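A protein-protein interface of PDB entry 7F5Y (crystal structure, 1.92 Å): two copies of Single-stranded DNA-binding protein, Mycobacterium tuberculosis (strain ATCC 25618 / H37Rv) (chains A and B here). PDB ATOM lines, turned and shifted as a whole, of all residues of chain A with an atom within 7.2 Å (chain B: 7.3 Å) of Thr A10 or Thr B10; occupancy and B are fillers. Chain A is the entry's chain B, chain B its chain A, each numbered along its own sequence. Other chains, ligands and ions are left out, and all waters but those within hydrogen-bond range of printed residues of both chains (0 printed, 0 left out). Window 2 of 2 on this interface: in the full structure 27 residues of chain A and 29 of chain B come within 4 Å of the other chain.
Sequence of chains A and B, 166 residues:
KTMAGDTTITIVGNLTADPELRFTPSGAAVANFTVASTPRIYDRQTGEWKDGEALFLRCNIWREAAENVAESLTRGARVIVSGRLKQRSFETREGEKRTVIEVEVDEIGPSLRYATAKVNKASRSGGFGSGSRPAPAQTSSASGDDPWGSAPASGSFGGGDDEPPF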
ATOM      1  N   THR A   8      32.376 -21.119 -17.434  1.00  0.00           N
ATOM      2  CA  THR A   8      31.861 -20.554 -16.190  1.00  0.00           C
ATOM      3  C   THR A   8      30.724 -19.564 -16.516  1.00  0.00           C
ATOM      4  O   THR A   8      30.576 -19.107 -17.619  1.00  0.00           O
ATOM      5  CB  THR A   8      32.990 -19.898 -15.391  1.00  0.00           C
ATOM      6  OG1 THR A   8      33.495 -18.839 -16.206  1.00  0.00           O
ATOM      7  CG2 THR A   8      34.084 -20.879 -15.026  1.00  0.00           C
ATOM      8  N   ILE A   9      29.867 -19.339 -15.529  1.00  0.00           N
ATOM      9  CA  ILE A   9      28.685 -18.534 -15.639  1.00  0.00           C
ATOM     10  C   ILE A   9      28.489 -17.919 -14.263  1.00  0.00           C
ATOM     11  O   ILE A   9      28.728 -18.585 -13.268  1.00  0.00           O
ATOM     12  CB  ILE A   9      27.481 -19.421 -16.036  1.00  0.00           C
ATOM     13  CG1 ILE A   9      26.158 -18.681 -16.012  1.00  0.00           C
ATOM     14  CG2 ILE A   9      27.373 -20.643 -15.138  1.00  0.00           C
ATOM     15  CD1 ILE A   9      25.027 -19.524 -16.544  1.00  0.00           C
ATOM     16  N   THR A  10      27.994 -16.699 -14.252  1.00  0.00           N
ATOM     17  CA  THR A  10      27.419 -16.064 -13.068  1.00  0.00           C
ATOM     18  C   THR A  10      25.938 -15.792 -13.323  1.00  0.00           C
ATOM     19  O   THR A  10      25.593 -15.206 -14.314  1.00  0.00           O
ATOM     20  CB  THR A  10      28.116 -14.742 -12.761  1.00  0.00           C
ATOM     21  OG1 THR A  10      29.445 -15.149 -12.432  1.00  0.00           O
ATOM     22  CG2 THR A  10      27.476 -14.001 -11.600  1.00  0.00           C
ATOM     23  N   ILE A  11      25.081 -16.255 -12.426  1.00  0.00           N
ATOM     24  CA  ILE A  11      23.667 -15.983 -12.571  1.00  0.00           C
ATOM     25  C   ILE A  11      23.153 -15.391 -11.261  1.00  0.00           C
ATOM     26  O   ILE A  11      23.564 -15.787 -10.161  1.00  0.00           O
ATOM     27  CB  ILE A  11      22.862 -17.205 -13.032  1.00  0.00           C
ATOM     28  CG1 ILE A  11      21.381 -16.848 -13.222  1.00  0.00           C
ATOM     29  CG2 ILE A  11      23.016 -18.375 -12.103  1.00  0.00           C
ATOM     30  CD1 ILE A  11      20.581 -17.880 -14.023  1.00  0.00           C
ATOM     31  N   VAL A  12      22.289 -14.391 -11.426  1.00  0.00           N
ATOM     32  CA  VAL A  12      21.619 -13.721 -10.380  1.00  0.00           C
ATOM     33  C   VAL A  12      20.121 -13.873 -10.574  1.00  0.00           C
ATOM     34  O   VAL A  12      19.587 -13.505 -11.592  1.00  0.00           O
ATOM     35  CB  VAL A  12      22.018 -12.228 -10.400  1.00  0.00           C
ATOM     36  CG1 VAL A  12      21.257 -11.448  -9.340  1.00  0.00           C
ATOM     37  CG2 VAL A  12      23.528 -12.027 -10.252  1.00  0.00           C
ATOM     38  N   LEU A  57      17.767 -21.808 -14.510  1.00  0.00           N
ATOM     39  CA  LEU A  57      18.902 -22.703 -14.591  1.00  0.00           C
ATOM     40  C   LEU A  57      18.874 -23.623 -13.380  1.00  0.00           C
ATOM     41  O   LEU A  57      18.784 -23.147 -12.251  1.00  0.00           O
ATOM     42  CB  LEU A  57      20.201 -21.875 -14.596  1.00  0.00           C
ATOM     43  CG  LEU A  57      20.527 -21.130 -15.887  1.00  0.00           C
ATOM     44  CD1 LEU A  57      21.890 -20.462 -15.790  1.00  0.00           C
ATOM     45  CD2 LEU A  57      20.507 -22.064 -17.080  1.00  0.00           C
ATOM     46  N   ILE A  80      23.294 -14.962  -5.792  1.00  0.00           N
ATOM     47  CA  ILE A  80      24.298 -14.801  -6.801  1.00  0.00           C
ATOM     48  C   ILE A  80      25.119 -16.099  -6.848  1.00  0.00           C
ATOM     49  O   ILE A  80      25.614 -16.545  -5.827  1.00  0.00           O
ATOM     50  CB  ILE A  80      25.145 -13.535  -6.555  1.00  0.00           C
ATOM     51  CG1 ILE A  80      26.362 -13.509  -7.490  1.00  0.00           C
ATOM     52  CG2 ILE A  80      25.531 -13.414  -5.091  1.00  0.00           C
ATOM     53  CD1 ILE A  80      27.069 -12.165  -7.571  1.00  0.00           C
ATOM     54  N   VAL A  81      25.174 -16.709  -8.038  1.00  0.00           N
ATOM     55  CA  VAL A  81      25.720 -18.009  -8.281  1.00  0.00           C
ATOM     56  C   VAL A  81      26.849 -17.887  -9.314  1.00  0.00           C
ATOM     57  O   VAL A  81      26.658 -17.392 -10.389  1.00  0.00           O
ATOM     58  CB  VAL A  81      24.623 -18.982  -8.728  1.00  0.00           C
ATOM     59  CG1 VAL A  81      25.179 -20.337  -9.106  1.00  0.00           C
ATOM     60  CG2 VAL A  81      23.628 -19.148  -7.617  1.00  0.00           C
ATOM     61  N   SER A  82      28.016 -18.428  -8.953  1.00  0.00           N
ATOM     62  CA  SER A  82      29.129 -18.595  -9.869  1.00  0.00           C
ATOM     63  C   SER A  82      29.375 -20.093 -10.015  1.00  0.00           C
ATOM     64  O   SER A  82      29.563 -20.779  -8.989  1.00  0.00           O
ATOM     65  CB  SER A  82      30.369 -17.934  -9.327  1.00  0.00           C
ATOM     66  OG  SER A  82      31.412 -18.154 -10.238  1.00  0.00           O
ATOM     67  N   GLY A  83      29.401 -20.590 -11.246  1.00  0.00           N
ATOM     68  CA  GLY A  83      29.650 -21.988 -11.451  1.00  0.00           C
ATOM     69  C   GLY A  83      30.004 -22.262 -12.882  1.00  0.00           C
ATOM     70  O   GLY A  83      30.407 -21.337 -13.613  1.00  0.00           O
ATOM     71  N   ARG A  84      29.870 -23.539 -13.239  1.00  0.00           N
ATOM     72  CA  ARG A  84      30.303 -24.083 -14.505  1.00  0.00           C
ATOM     73  C   ARG A  84      29.112 -24.766 -15.169  1.00  0.00           C
ATOM     74  O   ARG A  84      28.430 -25.569 -14.522  1.00  0.00           O
ATOM     75  CB  ARG A  84      31.441 -25.095 -14.296  1.00  0.00           C
ATOM     76  CG  ARG A  84      32.796 -24.432 -14.046  1.00  0.00           C
ATOM     77  CD  ARG A  84      33.798 -25.316 -13.330  1.00  0.00           C
ATOM     78  NE  ARG A  84      33.298 -25.750 -12.040  1.00  0.00           N
ATOM     79  CZ  ARG A  84      32.947 -26.996 -11.712  1.00  0.00           C
ATOM     80  NH1 ARG A  84      33.078 -28.006 -12.562  1.00  0.00           N
ATOM     81  NH2 ARG A  84      32.477 -27.215 -10.500  1.00  0.00           N
ATOM     82  N   VAL A 103      24.075 -25.953 -13.984  1.00  0.00           N
ATOM     83  CA  VAL A 103      25.173 -25.269 -13.320  1.00  0.00           C
ATOM     84  C   VAL A 103      25.682 -26.092 -12.128  1.00  0.00           C
ATOM     85  O   VAL A 103      24.953 -26.319 -11.154  1.00  0.00           O
ATOM     86  CB  VAL A 103      24.741 -23.870 -12.843  1.00  0.00           C
ATOM     87  CG1 VAL A 103      25.909 -23.172 -12.174  1.00  0.00           C
ATOM     88  CG2 VAL A 103      24.168 -23.007 -13.971  1.00  0.00           C
ATOM     89  N   THR B   8      32.142  -6.734 -17.498  1.00  0.00           N
ATOM     90  CA  THR B   8      31.603  -7.266 -16.276  1.00  0.00           C
ATOM     91  C   THR B   8      32.624  -8.240 -15.696  1.00  0.00           C
ATOM     92  O   THR B   8      33.426  -8.787 -16.412  1.00  0.00           O
ATOM     93  CB  THR B   8      30.296  -8.010 -16.550  1.00  0.00           C
ATOM     94  OG1 THR B   8      30.568  -8.937 -17.595  1.00  0.00           O
ATOM     95  CG2 THR B   8      29.177  -7.096 -16.975  1.00  0.00           C
ATOM     96  N   ILE B   9      32.635  -8.406 -14.379  1.00  0.00           N
ATOM     97  CA  ILE B   9      33.337  -9.526 -13.810  1.00  0.00           C
ATOM     98  C   ILE B   9      32.673  -9.931 -12.509  1.00  0.00           C
ATOM     99  O   ILE B   9      31.884  -9.209 -11.911  1.00  0.00           O
ATOM    100  CB  ILE B   9      34.849  -9.318 -13.568  1.00  0.00           C
ATOM    101  CG1 ILE B   9      35.139  -8.193 -12.577  1.00  0.00           C
ATOM    102  CG2 ILE B   9      35.626  -9.194 -14.870  1.00  0.00           C
ATOM    103  CD1 ILE B   9      36.434  -8.388 -11.805  1.00  0.00           C
ATOM    104  N   THR B  10      33.075 -11.129 -12.122  1.00  0.00           N
ATOM    105  CA  THR B  10      32.709 -11.762 -10.908  1.00  0.00           C
ATOM    106  C   THR B  10      33.999 -12.023 -10.135  1.00  0.00           C
ATOM    107  O   THR B  10      34.920 -12.564 -10.670  1.00  0.00           O
ATOM    108  CB  THR B  10      32.014 -13.102 -11.155  1.00  0.00           C
ATOM    109  OG1 THR B  10      30.813 -12.745 -11.809  1.00  0.00           O
ATOM    110  CG2 THR B  10      31.702 -13.865  -9.886  1.00  0.00           C
ATOM    111  N   ILE B  11      34.063 -11.536  -8.908  1.00  0.00           N
ATOM    112  CA  ILE B  11      35.216 -11.815  -8.076  1.00  0.00           C
ATOM    113  C   ILE B  11      34.722 -12.434  -6.779  1.00  0.00           C
ATOM    114  O   ILE B  11      33.686 -12.066  -6.239  1.00  0.00           O
ATOM    115  CB  ILE B  11      36.108 -10.566  -7.880  1.00  0.00           C
ATOM    116  CG1 ILE B  11      37.315 -10.862  -6.986  1.00  0.00           C
ATOM    117  CG2 ILE B  11      35.338  -9.346  -7.405  1.00  0.00           C
ATOM    118  CD1 ILE B  11      38.342  -9.754  -6.945  1.00  0.00           C
ATOM    119  N   VAL B  12      35.454 -13.471  -6.368  1.00  0.00           N
ATOM    120  CA  VAL B  12      35.291 -14.126  -5.085  1.00  0.00           C
ATOM    121  C   VAL B  12      36.553 -13.935  -4.270  1.00  0.00           C
ATOM    122  O   VAL B  12      37.616 -14.221  -4.756  1.00  0.00           O
ATOM    123  CB  VAL B  12      35.045 -15.625  -5.299  1.00  0.00           C
ATOM    124  CG1 VAL B  12      34.948 -16.376  -3.983  1.00  0.00           C
ATOM    125  CG2 VAL B  12      33.823 -15.849  -6.147  1.00  0.00           C
ATOM    126  N   LEU B  57      40.783  -5.697  -5.533  1.00  0.00           N
ATOM    127  CA  LEU B  57      39.906  -4.825  -6.283  1.00  0.00           C
ATOM    128  C   LEU B  57      39.062  -3.982  -5.332  1.00  0.00           C
ATOM    129  O   LEU B  57      38.252  -4.506  -4.584  1.00  0.00           O
ATOM    130  CB  LEU B  57      39.000  -5.651  -7.199  1.00  0.00           C
ATOM    131  CG  LEU B  57      39.670  -6.212  -8.438  1.00  0.00           C
ATOM    132  CD1 LEU B  57      38.707  -7.073  -9.238  1.00  0.00           C
ATOM    133  CD2 LEU B  57      40.199  -5.090  -9.313  1.00  0.00           C
ATOM    134  N   ILE B  80      30.975 -12.911  -2.851  1.00  0.00           N
ATOM    135  CA  ILE B  80      30.889 -13.016  -4.287  1.00  0.00           C
ATOM    136  C   ILE B  80      30.239 -11.724  -4.807  1.00  0.00           C
ATOM    137  O   ILE B  80      29.156 -11.324  -4.375  1.00  0.00           O
ATOM    138  CB  ILE B  80      30.159 -14.299  -4.743  1.00  0.00           C
ATOM    139  CG1 ILE B  80      29.774 -14.222  -6.223  1.00  0.00           C
ATOM    140  CG2 ILE B  80      28.953 -14.593  -3.874  1.00  0.00           C
ATOM    141  CD1 ILE B  80      29.325 -15.540  -6.810  1.00  0.00           C
ATOM    142  N   VAL B  81      30.960 -11.083  -5.725  1.00  0.00           N
ATOM    143  CA  VAL B  81      30.715  -9.763  -6.187  1.00  0.00           C
ATOM    144  C   VAL B  81      30.601  -9.844  -7.696  1.00  0.00           C
ATOM    145  O   VAL B  81      31.546 -10.292  -8.379  1.00  0.00           O
ATOM    146  CB  VAL B  81      31.837  -8.788  -5.803  1.00  0.00           C
ATOM    147  CG1 VAL B  81      31.649  -7.431  -6.461  1.00  0.00           C
ATOM    148  CG2 VAL B  81      32.015  -8.655  -4.298  1.00  0.00           C
ATOM    149  N   SER B  82      29.461  -9.377  -8.196  1.00  0.00           N
ATOM    150  CA  SER B  82      29.283  -9.187  -9.616  1.00  0.00           C
ATOM    151  C   SER B  82      29.152  -7.686  -9.934  1.00  0.00           C
ATOM    152  O   SER B  82      28.457  -6.964  -9.284  1.00  0.00           O
ATOM    153  CB  SER B  82      28.081  -9.959 -10.063  1.00  0.00           C
ATOM    154  OG  SER B  82      27.829  -9.694 -11.415  1.00  0.00           O
ATOM    155  N   GLY B  83      29.881  -7.209 -10.918  1.00  0.00           N
ATOM    156  CA  GLY B  83      29.821  -5.802 -11.279  1.00  0.00           C
ATOM    157  C   GLY B  83      30.511  -5.534 -12.592  1.00  0.00           C
ATOM    158  O   GLY B  83      30.694  -6.457 -13.411  1.00  0.00           O
ATOM    159  N   ARG B  84      30.876  -4.268 -12.794  1.00  0.00           N
ATOM    160  CA  ARG B  84      31.417  -3.760 -14.031  1.00  0.00           C
ATOM    161  C   ARG B  84      32.707  -3.027 -13.690  1.00  0.00           C
ATOM    162  O   ARG B  84      32.735  -2.242 -12.694  1.00  0.00           O
ATOM    163  CB  ARG B  84      30.456  -2.749 -14.676  1.00  0.00           C
ATOM    164  CG  ARG B  84      29.200  -3.381 -15.261  1.00  0.00           C
ATOM    165  CD  ARG B  84      28.062  -2.381 -15.425  1.00  0.00           C
ATOM    166  NE  ARG B  84      27.493  -2.004 -14.139  1.00  0.00           N
ATOM    167  CZ  ARG B  84      27.535  -0.795 -13.611  1.00  0.00           C
ATOM    168  NH1 ARG B  84      28.015   0.221 -14.311  1.00  0.00           N
ATOM    169  NH2 ARG B  84      27.090  -0.613 -12.378  1.00  0.00           N
ATOM    170  N   VAL B 103      35.644  -1.578  -9.381  1.00  0.00           N
ATOM    171  CA  VAL B 103      34.464  -2.363  -9.602  1.00  0.00           C
ATOM    172  C   VAL B 103      33.239  -1.582  -9.119  1.00  0.00           C
ATOM    173  O   VAL B 103      33.106  -1.252  -7.976  1.00  0.00           O
ATOM    174  CB  VAL B 103      34.559  -3.741  -8.915  1.00  0.00           C
ATOM    175  CG1 VAL B 103      33.281  -4.572  -9.157  1.00  0.00           C
ATOM    176  CG2 VAL B 103      35.779  -4.502  -9.375  1.00  0.00           C
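Of the 12 printed residues of chain A, 3 touch a printed residue of chain B. Printed residues of chain A that touch a printed residue of chain B: Thr A10, Ile A80 and Ser A82. Hydrophobic or aromatic side chains of chain A within 4 Å of the printed part of chain B: Ile A80. Among the printed residues, no Asp or Glu carboxylate lies within 4 Å of a Lys or Arg side-chain nitrogen of the other chain.
The side-chain hydroxyl (OG1) of Thr A10 lies within hydrogen-bond range of the side-chain hydroxyl (OG1) of Thr B10 (2.8 Å).
Thr B10 touches its own counterpart, Thr A10. Ile A80 touches its own counterpart, Ile B80. Ile A80 touches Ser B82, and with the chains exchanged Ser A82 touches Ile B80. 12 positions are printed for both chains. Of the 4 pairs that touch across the chains among the printed residues, 4 have their exchanged pair printed and touching as well.
Thr A10 touches just one residue of chain B: Thr B10. Of chain A, only Thr A10 (2.8 Å) comes within 4 Å of Thr B10. Printed residues of chain A within 4 Å of Ser B82: Ile A80 (3.5 Å). Printed residues of chain B within 4 Å of Ser A82: Ile B80. Of the printed residues of chain B, Ile A80 touches Ile B80 (3.7 Å) and Ser B82 (3.5 Å). Printed residues of chain A within 4 Å of Ile B80: Ile A80 and Ser A82. The nearest residue of chain A that does not touch Thr B10 is Ser A82 (4.3 Å).
Among the printed residues, pairs that only touch across the chains: Ile A80 with Ser B82, Ser A82 with Ile B80 and Ile A80 with Ile B80.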
